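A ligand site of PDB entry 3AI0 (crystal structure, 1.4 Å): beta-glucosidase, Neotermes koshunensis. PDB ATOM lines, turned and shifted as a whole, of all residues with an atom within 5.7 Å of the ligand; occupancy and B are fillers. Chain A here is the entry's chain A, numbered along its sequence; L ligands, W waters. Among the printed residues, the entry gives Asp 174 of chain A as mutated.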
ATOM      1  N   ALA A  23     -21.191  22.999 -12.908  1.00  0.00           N
ATOM      2  CA  ALA A  23     -22.000  21.916 -12.331  1.00  0.00           C
ATOM      3  C   ALA A  23     -21.623  20.581 -12.973  1.00  0.00           C
ATOM      4  O   ALA A  23     -21.370  20.517 -14.178  1.00  0.00           O
ATOM      5  CB  ALA A  23     -23.494  22.186 -12.496  1.00  0.00           C
ATOM      6  N   GLN A  26     -23.329  19.108 -16.098  1.00  0.00           N
ATOM      7  CA  GLN A  26     -23.153  20.015 -17.221  1.00  0.00           C
ATOM      8  C   GLN A  26     -21.768  19.932 -17.874  1.00  0.00           C
ATOM      9  O   GLN A  26     -21.622  20.296 -19.048  1.00  0.00           O
ATOM     10  CB  GLN A  26     -23.439  21.456 -16.793  1.00  0.00           C
ATOM     11  CG  GLN A  26     -24.874  21.561 -16.281  1.00  0.00           C
ATOM     12  CD  GLN A  26     -25.317  23.005 -16.109  1.00  0.00           C
ATOM     13  OE1 GLN A  26     -25.257  23.550 -15.008  1.00  0.00           O
ATOM     14  NE2 GLN A  26     -25.691  23.640 -17.216  1.00  0.00           N
ATOM     15  N   HIS A 129     -26.411  19.672  -7.402  1.00  0.00           N
ATOM     16  CA  HIS A 129     -26.851  20.504  -8.517  1.00  0.00           C
ATOM     17  C   HIS A 129     -27.632  19.679  -9.547  1.00  0.00           C
ATOM     18  O   HIS A 129     -27.276  19.593 -10.722  1.00  0.00           O
ATOM     19  CB  HIS A 129     -25.667  21.263  -9.136  1.00  0.00           C
ATOM     20  CG  HIS A 129     -26.036  22.443  -9.998  1.00  0.00           C
ATOM     21  ND1 HIS A 129     -25.278  23.601 -10.010  1.00  0.00           N
ATOM     22  CD2 HIS A 129     -26.989  22.618 -10.947  1.00  0.00           C
ATOM     23  CE1 HIS A 129     -25.728  24.409 -10.955  1.00  0.00           C
ATOM     24  NE2 HIS A 129     -26.808  23.869 -11.490  1.00  0.00           N
ATOM     25  N   TRP A 130     -28.673  19.002  -9.053  1.00  0.00           N
ATOM     26  CA  TRP A 130     -29.802  18.489  -9.843  1.00  0.00           C
ATOM     27  C   TRP A 130     -29.685  17.032 -10.296  1.00  0.00           C
ATOM     28  O   TRP A 130     -30.626  16.523 -10.903  1.00  0.00           O
ATOM     29  CB  TRP A 130     -30.187  19.381 -11.041  1.00  0.00           C
ATOM     30  CG  TRP A 130     -30.404  20.847 -10.719  1.00  0.00           C
ATOM     31  CD1 TRP A 130     -30.397  21.468  -9.484  1.00  0.00           C
ATOM     32  CD2 TRP A 130     -30.740  21.866 -11.666  1.00  0.00           C
ATOM     33  NE1 TRP A 130     -30.709  22.802  -9.629  1.00  0.00           N
ATOM     34  CE2 TRP A 130     -30.950  23.072 -10.955  1.00  0.00           C
ATOM     35  CE3 TRP A 130     -30.895  21.869 -13.071  1.00  0.00           C
ATOM     36  CZ2 TRP A 130     -31.267  24.281 -11.586  1.00  0.00           C
ATOM     37  CZ3 TRP A 130     -31.230  23.059 -13.687  1.00  0.00           C
ATOM     38  CH2 TRP A 130     -31.417  24.243 -12.950  1.00  0.00           C
ATOM     39  N   ASN A 173     -28.176  23.490  -4.827  1.00  0.00           N
ATOM     40  CA  ASN A 173     -28.275  24.552  -5.803  1.00  0.00           C
ATOM     41  C   ASN A 173     -29.714  24.677  -6.312  1.00  0.00           C
ATOM     42  O   ASN A 173     -30.200  23.781  -7.004  1.00  0.00           O
ATOM     43  CB  ASN A 173     -27.367  24.341  -7.015  1.00  0.00           C
ATOM     44  CG  ASN A 173     -27.311  25.588  -7.861  1.00  0.00           C
ATOM     45  OD1 ASN A 173     -26.744  26.596  -7.437  1.00  0.00           O
ATOM     46  ND2 ASN A 173     -27.866  25.526  -9.065  1.00  0.00           N
ATOM     47  N   ASP A 174     -30.350  25.800  -5.993  1.00  0.00           N
ATOM     48  CA  ASP A 174     -31.640  26.192  -6.587  1.00  0.00           C
ATOM     49  C   ASP A 174     -32.731  25.118  -6.570  1.00  0.00           C
ATOM     50  O   ASP A 174     -33.160  24.610  -7.625  1.00  0.00           O
ATOM     51  CB  ASP A 174     -31.395  26.686  -8.013  1.00  0.00           C
ATOM     52  CG  ASP A 174     -32.630  27.289  -8.662  1.00  0.00           C
ATOM     53  OD1 ASP A 174     -33.660  27.501  -7.960  1.00  0.00           O
ATOM     54  OD2 ASP A 174     -32.568  27.535  -9.896  1.00  0.00           O
ATOM     55  N   THR A 177     -35.983  25.778  -8.727  1.00  0.00           N
ATOM     56  CA  THR A 177     -36.054  25.199 -10.056  1.00  0.00           C
ATOM     57  C   THR A 177     -36.149  23.670 -10.040  1.00  0.00           C
ATOM     58  O   THR A 177     -36.991  23.112 -10.734  1.00  0.00           O
ATOM     59  CB  THR A 177     -34.844  25.635 -10.918  1.00  0.00           C
ATOM     60  OG1 THR A 177     -34.876  27.063 -11.030  1.00  0.00           O
ATOM     61  CG2 THR A 177     -34.879  25.025 -12.311  1.00  0.00           C
ATOM     62  N   ASN A 234     -32.107  30.651  -6.118  1.00  0.00           N
ATOM     63  CA  ASN A 234     -32.290  31.465  -7.319  1.00  0.00           C
ATOM     64  C   ASN A 234     -33.492  32.384  -7.125  1.00  0.00           C
ATOM     65  O   ASN A 234     -34.571  31.934  -6.746  1.00  0.00           O
ATOM     66  CB  ASN A 234     -32.472  30.556  -8.537  1.00  0.00           C
ATOM     67  CG  ASN A 234     -32.477  31.333  -9.855  1.00  0.00           C
ATOM     68  OD1 ASN A 234     -33.384  32.137 -10.093  1.00  0.00           O
ATOM     69  ND2 ASN A 234     -31.513  31.031 -10.735  1.00  0.00           N
ATOM     70  N   ASN A 236     -35.273  36.135  -9.105  1.00  0.00           N
ATOM     71  CA  ASN A 236     -35.245  37.289  -9.983  1.00  0.00           C
ATOM     72  C   ASN A 236     -35.839  38.506  -9.283  1.00  0.00           C
ATOM     73  O   ASN A 236     -36.635  38.365  -8.355  1.00  0.00           O
ATOM     74  CB  ASN A 236     -36.069  36.980 -11.215  1.00  0.00           C
ATOM     75  CG  ASN A 236     -35.374  35.954 -12.077  1.00  0.00           C
ATOM     76  OD1 ASN A 236     -34.168  36.017 -12.320  1.00  0.00           O
ATOM     77  ND2 ASN A 236     -36.145  34.958 -12.473  1.00  0.00           N
ATOM     78  N   TYR A 254     -44.543  37.421  -5.064  1.00  0.00           N
ATOM     79  CA  TYR A 254     -43.493  36.749  -5.845  1.00  0.00           C
ATOM     80  C   TYR A 254     -42.261  36.459  -5.000  1.00  0.00           C
ATOM     81  O   TYR A 254     -41.751  35.325  -4.994  1.00  0.00           O
ATOM     82  CB  TYR A 254     -43.115  37.594  -7.077  1.00  0.00           C
ATOM     83  CG  TYR A 254     -41.919  37.027  -7.793  1.00  0.00           C
ATOM     84  CD1 TYR A 254     -42.040  35.997  -8.725  1.00  0.00           C
ATOM     85  CD2 TYR A 254     -40.632  37.478  -7.485  1.00  0.00           C
ATOM     86  CE1 TYR A 254     -40.877  35.439  -9.301  1.00  0.00           C
ATOM     87  CE2 TYR A 254     -39.492  36.939  -8.056  1.00  0.00           C
ATOM     88  CZ  TYR A 254     -39.616  35.930  -8.982  1.00  0.00           C
ATOM     89  OH  TYR A 254     -38.410  35.415  -9.442  1.00  0.00           O
ATOM     90  N   ASN A 316     -28.314  32.916  -6.738  1.00  0.00           N
ATOM     91  CA  ASN A 316     -28.211  32.797  -8.185  1.00  0.00           C
ATOM     92  C   ASN A 316     -29.172  33.836  -8.756  1.00  0.00           C
ATOM     93  O   ASN A 316     -30.379  33.775  -8.503  1.00  0.00           O
ATOM     94  CB  ASN A 316     -28.635  31.395  -8.645  1.00  0.00           C
ATOM     95  CG  ASN A 316     -27.726  30.298  -8.114  1.00  0.00           C
ATOM     96  OD1 ASN A 316     -26.676  30.589  -7.524  1.00  0.00           O
ATOM     97  ND2 ASN A 316     -28.104  29.042  -8.329  1.00  0.00           N
ATOM     98  N   TYR A 318     -30.220  36.134 -12.299  1.00  0.00           N
ATOM     99  CA  TYR A 318     -30.039  36.272 -13.749  1.00  0.00           C
ATOM    100  C   TYR A 318     -30.830  37.413 -14.376  1.00  0.00           C
ATOM    101  O   TYR A 318     -30.366  38.018 -15.354  1.00  0.00           O
ATOM    102  CB  TYR A 318     -30.413  34.988 -14.480  1.00  0.00           C
ATOM    103  CG  TYR A 318     -29.469  33.829 -14.283  1.00  0.00           C
ATOM    104  CD1 TYR A 318     -29.509  33.034 -13.148  1.00  0.00           C
ATOM    105  CD2 TYR A 318     -28.496  33.541 -15.238  1.00  0.00           C
ATOM    106  CE1 TYR A 318     -28.610  31.991 -12.959  1.00  0.00           C
ATOM    107  CE2 TYR A 318     -27.644  32.472 -15.086  1.00  0.00           C
ATOM    108  CZ  TYR A 318     -27.693  31.676 -13.952  1.00  0.00           C
ATOM    109  OH  TYR A 318     -26.831  30.610 -13.841  1.00  0.00           O
ATOM    110  N   THR A 319     -32.059  37.644 -13.924  1.00  0.00           N
ATOM    111  CA  THR A 319     -32.974  38.511 -14.680  1.00  0.00           C
ATOM    112  C   THR A 319     -34.044  39.170 -13.814  1.00  0.00           C
ATOM    113  O   THR A 319     -33.953  39.139 -12.581  1.00  0.00           O
ATOM    114  CB  THR A 319     -33.555  37.722 -15.883  1.00  0.00           C
ATOM    115  OG1 THR A 319     -34.136  38.611 -16.854  1.00  0.00           O
ATOM    116  CG2 THR A 319     -34.552  36.639 -15.469  1.00  0.00           C
ATOM    117  N   SER A 353     -31.713  33.018 -24.445  1.00  0.00           N
ATOM    118  CA  SER A 353     -32.645  32.233 -23.633  1.00  0.00           C
ATOM    119  C   SER A 353     -33.934  33.051 -23.472  1.00  0.00           C
ATOM    120  O   SER A 353     -33.891  34.211 -23.047  1.00  0.00           O
ATOM    121  CB  SER A 353     -32.062  31.970 -22.241  1.00  0.00           C
ATOM    122  OG  SER A 353     -30.791  31.351 -22.294  1.00  0.00           O
ATOM    123  N   TRP A 355     -36.225  33.301 -21.402  1.00  0.00           N
ATOM    124  CA  TRP A 355     -36.565  33.787 -20.071  1.00  0.00           C
ATOM    125  C   TRP A 355     -35.592  34.839 -19.545  1.00  0.00           C
ATOM    126  O   TRP A 355     -35.855  35.473 -18.511  1.00  0.00           O
ATOM    127  CB  TRP A 355     -36.559  32.585 -19.108  1.00  0.00           C
ATOM    128  CG  TRP A 355     -35.275  31.789 -19.131  1.00  0.00           C
ATOM    129  CD1 TRP A 355     -34.985  30.682 -19.902  1.00  0.00           C
ATOM    130  CD2 TRP A 355     -34.093  32.055 -18.364  1.00  0.00           C
ATOM    131  NE1 TRP A 355     -33.712  30.232 -19.634  1.00  0.00           N
ATOM    132  CE2 TRP A 355     -33.132  31.070 -18.709  1.00  0.00           C
ATOM    133  CE3 TRP A 355     -33.752  33.015 -17.407  1.00  0.00           C
ATOM    134  CZ2 TRP A 355     -31.850  31.064 -18.183  1.00  0.00           C
ATOM    135  CZ3 TRP A 355     -32.469  33.000 -16.879  1.00  0.00           C
ATOM    136  CH2 TRP A 355     -31.531  32.042 -17.272  1.00  0.00           C
ATOM    137  N   GLU A 383     -24.182  32.228  -8.793  1.00  0.00           N
ATOM    138  CA  GLU A 383     -24.367  32.236 -10.252  1.00  0.00           C
ATOM    139  C   GLU A 383     -24.877  33.594 -10.720  1.00  0.00           C
ATOM    140  O   GLU A 383     -25.762  34.185 -10.107  1.00  0.00           O
ATOM    141  CB  GLU A 383     -25.415  31.215 -10.737  1.00  0.00           C
ATOM    142  CG  GLU A 383     -25.071  29.765 -10.441  1.00  0.00           C
ATOM    143  CD  GLU A 383     -26.111  28.749 -10.866  1.00  0.00           C
ATOM    144  OE1 GLU A 383     -26.958  29.027 -11.740  1.00  0.00           O
ATOM    145  OE2 GLU A 383     -25.961  27.598 -10.380  1.00  0.00           O
ATOM    146  N   TRP A 425     -21.146  32.639 -13.699  1.00  0.00           N
ATOM    147  CA  TRP A 425     -21.674  31.433 -14.323  1.00  0.00           C
ATOM    148  C   TRP A 425     -21.587  31.607 -15.837  1.00  0.00           C
ATOM    149  O   TRP A 425     -22.183  32.546 -16.367  1.00  0.00           O
ATOM    150  CB  TRP A 425     -23.165  31.290 -13.962  1.00  0.00           C
ATOM    151  CG  TRP A 425     -23.671  29.978 -14.478  1.00  0.00           C
ATOM    152  CD1 TRP A 425     -24.346  29.755 -15.641  1.00  0.00           C
ATOM    153  CD2 TRP A 425     -23.423  28.684 -13.903  1.00  0.00           C
ATOM    154  NE1 TRP A 425     -24.540  28.402 -15.834  1.00  0.00           N
ATOM    155  CE2 TRP A 425     -23.988  27.727 -14.770  1.00  0.00           C
ATOM    156  CE3 TRP A 425     -22.742  28.240 -12.763  1.00  0.00           C
ATOM    157  CZ2 TRP A 425     -23.926  26.357 -14.516  1.00  0.00           C
ATOM    158  CZ3 TRP A 425     -22.700  26.869 -12.499  1.00  0.00           C
ATOM    159  CH2 TRP A 425     -23.312  25.960 -13.358  1.00  0.00           C
ATOM    160  N   ASN A 430     -21.699  24.696 -21.689  1.00  0.00           N
ATOM    161  CA  ASN A 430     -22.212  23.562 -20.911  1.00  0.00           C
ATOM    162  C   ASN A 430     -23.174  22.697 -21.705  1.00  0.00           C
ATOM    163  O   ASN A 430     -23.742  23.182 -22.685  1.00  0.00           O
ATOM    164  CB  ASN A 430     -23.134  24.049 -19.753  1.00  0.00           C
ATOM    165  CG  ASN A 430     -22.409  24.927 -18.778  1.00  0.00           C
ATOM    166  OD1 ASN A 430     -21.350  24.543 -18.290  1.00  0.00           O
ATOM    167  ND2 ASN A 430     -22.960  26.096 -18.486  1.00  0.00           N
ATOM    168  N   GLU A 432     -26.646  22.440 -21.384  1.00  0.00           N
ATOM    169  CA  GLU A 432     -27.605  23.367 -20.759  1.00  0.00           C
ATOM    170  C   GLU A 432     -28.969  22.731 -20.536  1.00  0.00           C
ATOM    171  O   GLU A 432     -30.011  23.271 -20.895  1.00  0.00           O
ATOM    172  CB  GLU A 432     -27.715  24.646 -21.600  1.00  0.00           C
ATOM    173  CG  GLU A 432     -26.514  25.543 -21.418  1.00  0.00           C
ATOM    174  CD  GLU A 432     -26.335  26.140 -20.026  1.00  0.00           C
ATOM    175  OE1 GLU A 432     -27.231  26.072 -19.130  1.00  0.00           O
ATOM    176  OE2 GLU A 432     -25.191  26.626 -19.845  1.00  0.00           O
ATOM    177  N   TRP A 433     -28.955  21.589 -19.854  1.00  0.00           N
ATOM    178  CA  TRP A 433     -30.201  20.948 -19.450  1.00  0.00           C
ATOM    179  C   TRP A 433     -31.106  20.723 -20.675  1.00  0.00           C
ATOM    180  O   TRP A 433     -30.649  20.144 -21.671  1.00  0.00           O
ATOM    181  CB  TRP A 433     -30.832  21.757 -18.310  1.00  0.00           C
ATOM    182  CG  TRP A 433     -29.877  22.009 -17.171  1.00  0.00           C
ATOM    183  CD1 TRP A 433     -29.439  23.230 -16.740  1.00  0.00           C
ATOM    184  CD2 TRP A 433     -29.231  21.024 -16.330  1.00  0.00           C
ATOM    185  NE1 TRP A 433     -28.583  23.082 -15.669  1.00  0.00           N
ATOM    186  CE2 TRP A 433     -28.443  21.735 -15.396  1.00  0.00           C
ATOM    187  CE3 TRP A 433     -29.284  19.632 -16.240  1.00  0.00           C
ATOM    188  CZ2 TRP A 433     -27.693  21.092 -14.391  1.00  0.00           C
ATOM    189  CZ3 TRP A 433     -28.542  18.975 -15.243  1.00  0.00           C
ATOM    190  CH2 TRP A 433     -27.769  19.723 -14.319  1.00  0.00           C
ATOM    191  N   GLU A 439     -27.498  26.687 -26.255  1.00  0.00           N
ATOM    192  CA  GLU A 439     -27.284  27.970 -25.573  1.00  0.00           C
ATOM    193  C   GLU A 439     -25.904  27.963 -24.929  1.00  0.00           C
ATOM    194  O   GLU A 439     -25.526  26.979 -24.296  1.00  0.00           O
ATOM    195  CB  GLU A 439     -28.397  28.236 -24.548  1.00  0.00           C
ATOM    196  CG  GLU A 439     -29.757  28.323 -25.219  1.00  0.00           C
ATOM    197  CD  GLU A 439     -30.917  28.488 -24.245  1.00  0.00           C
ATOM    198  OE1 GLU A 439     -32.075  28.305 -24.670  1.00  0.00           O
ATOM    199  OE2 GLU A 439     -30.664  28.778 -23.056  1.00  0.00           O
ATOM    200  N   PHE A 441     -23.409  29.717 -22.220  1.00  0.00           N
ATOM    201  CA  PHE A 441     -23.265  30.526 -21.011  1.00  0.00           C
ATOM    202  C   PHE A 441     -21.822  30.689 -20.557  1.00  0.00           C
ATOM    203  O   PHE A 441     -21.560  31.315 -19.527  1.00  0.00           O
ATOM    204  CB  PHE A 441     -24.083  29.974 -19.837  1.00  0.00           C
ATOM    205  CG  PHE A 441     -25.542  30.340 -19.878  1.00  0.00           C
ATOM    206  CD1 PHE A 441     -26.019  31.423 -19.152  1.00  0.00           C
ATOM    207  CD2 PHE A 441     -26.435  29.561 -20.606  1.00  0.00           C
ATOM    208  CE1 PHE A 441     -27.383  31.755 -19.171  1.00  0.00           C
ATOM    209  CE2 PHE A 441     -27.779  29.895 -20.625  1.00  0.00           C
ATOM    210  CZ  PHE A 441     -28.266  30.969 -19.887  1.00  0.00           C
HETATM  211  C1  LIG L   1     -29.541  28.049 -14.005  1.00  0.00           C
HETATM  212  N1  LIG L   1     -34.557  32.030 -13.452  1.00  0.00           N
HETATM  213  O1  LIG L   1     -30.871  27.890 -13.530  1.00  0.00           O
HETATM  214  C2  LIG L   1     -28.800  26.781 -13.587  1.00  0.00           C
HETATM  215  O2  LIG L   1     -28.479  26.826 -12.195  1.00  0.00           O
HETATM  216  C3  LIG L   1     -27.520  26.518 -14.378  1.00  0.00           C
HETATM  217  O3  LIG L   1     -27.185  25.144 -14.151  1.00  0.00           O
HETATM  218  C4  LIG L   1     -27.825  26.752 -15.864  1.00  0.00           C
HETATM  219  O4  LIG L   1     -26.601  26.593 -16.579  1.00  0.00           O
HETATM  220  C5  LIG L   1     -28.370  28.176 -16.030  1.00  0.00           C
HETATM  221  O5  LIG L   1     -29.668  28.144 -15.429  1.00  0.00           O
HETATM  222  C6  LIG L   1     -28.589  28.605 -17.484  1.00  0.00           C
HETATM  223  O6  LIG L   1     -29.351  27.670 -18.242  1.00  0.00           O
HETATM  224  C7  LIG L   1     -31.744  28.944 -13.556  1.00  0.00           C
HETATM  225  O7  LIG L   1     -35.623  31.847 -12.867  1.00  0.00           O
HETATM  226  C8  LIG L   1     -32.988  28.736 -12.984  1.00  0.00           C
HETATM  227  O8  LIG L   1     -34.324  33.109 -13.964  1.00  0.00           O
HETATM  228  C9  LIG L   1     -33.921  29.775 -12.907  1.00  0.00           C
HETATM  229  C10 LIG L   1     -33.605  31.000 -13.500  1.00  0.00           C
HETATM  230  C11 LIG L   1     -32.332  31.217 -14.052  1.00  0.00           C
HETATM  231  C12 LIG L   1     -31.400  30.182 -14.109  1.00  0.00           C
HETATM  232  O   HOH W   1     -31.762  26.265 -16.591  1.00  0.00           O
HETATM  233  O   HOH W   2     -31.417  25.403 -19.304  1.00  0.00           O
HETATM  234  O   HOH W   3     -35.834  31.851  -9.736  1.00  0.00           O
HETATM  235  O   HOH W   4     -32.426  34.169 -11.732  1.00  0.00           O
HETATM  236  O   HOH W   5     -31.353  28.085 -20.303  1.00  0.00           O
HETATM  237  O   HOH W   6     -30.108  28.471 -10.442  1.00  0.00           O
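Trp 130 touches the ligand. Asp 174 touches the ligand. Thr 177 touches the ligand. Asn 234 touches the ligand. CD1 of Tyr 318 touches C11 of the ligand, 3.5 Å away. Thr 319 touches the ligand (CG2 to O8, 3.8 Å). Trp 355 touches the ligand. Phe 441 touches the ligand. Hydrophobic or aromatic side chains that line the ligand: His 129, Trp 130, Tyr 318, Trp 355, Trp 425, Trp 433 and Phe 441. Of the 22 residues printed, 16 come within 4 Å of the ligand. The nearest printed residue that does not touch the ligand is Asn 430 (4.1 Å).
N of Asn 236 lies within hydrogen-bond range of OH of Tyr 254 (3.2 Å). The side-chain amide oxygen (OD1) of Asn 236 is in hydrogen-bond range of the backbone NH (N) of Thr 319, at 3.1 Å. The side-chain carboxylate of Asp 174 lies within hydrogen-bond range of the side-chain hydroxyl of Thr 177, at 2.6 Å. The side-chain amide oxygen of Asn 173 lies within hydrogen-bond range of the side-chain amide nitrogen of Asn 316. The side-chain carboxylate of Glu 432 sits at hydrogen-bond distance from the side-chain amide nitrogen of Asn 430, at 2.7 Å. The indole nitrogen of Trp 433 sits close to the side-chain amide nitrogen of Gln 26. The side-chain hydroxyl (OH) of Tyr 318 is in hydrogen-bond range of the side-chain carboxylate (OE1) of Glu 383. The side-chain amide oxygen of Asn 316 sits at hydrogen-bond distance from the backbone NH of Glu 383 (3.2 Å).
Water W5 lies within hydrogen-bond range of an oxygen (O6) of the ligand, the side-chain carboxylate of Glu 439 and the indole nitrogen of Trp 355. Water W6 lies within hydrogen-bond range of the side-chain carboxylate of Asp 174 (2.7 Å), an oxygen (O2) of the ligand (2.9 Å), the side-chain amide nitrogen of Asn 234 (2.9 Å), the side-chain amide nitrogen of Asn 316 (3.0 Å) and the side-chain carboxylate of Glu 383 (3.5 Å). Water W3 bridges the side-chain amide oxygen (OD1) of Asn 234 (2.5 Å) and an oxygen (O7) of the ligand (3.1 Å). Water W2 bridges O of Glu 432 and O6 of the ligand.
An oxygen (O4) of the ligand is in hydrogen-bond range of the side-chain carboxylate (OE1) of Glu 432 (2.7 Å). O2 of the ligand lies within hydrogen-bond range of ND2 of Asn 173. An oxygen (O8) of the ligand lies within hydrogen-bond range of the side-chain amide nitrogen of Asn 236 (3.0 Å). The side-chain amide oxygen (OE1) of Gln 26 lies within hydrogen-bond range of an oxygen (O3) of the ligand (2.6 Å). An oxygen (O2) of the ligand is in hydrogen-bond range of the side-chain carboxylate (OE1) of Glu 383 (2.7 Å). NE2 of His 129 is in hydrogen-bond range of O3 of the ligand (3.0 Å). NE1 of Trp 433 lies within hydrogen-bond range of O3 of the ligand. The indole nitrogen (NE1) of Trp 425 lies within hydrogen-bond range of an oxygen (O4) of the ligand, 2.8 Å away.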
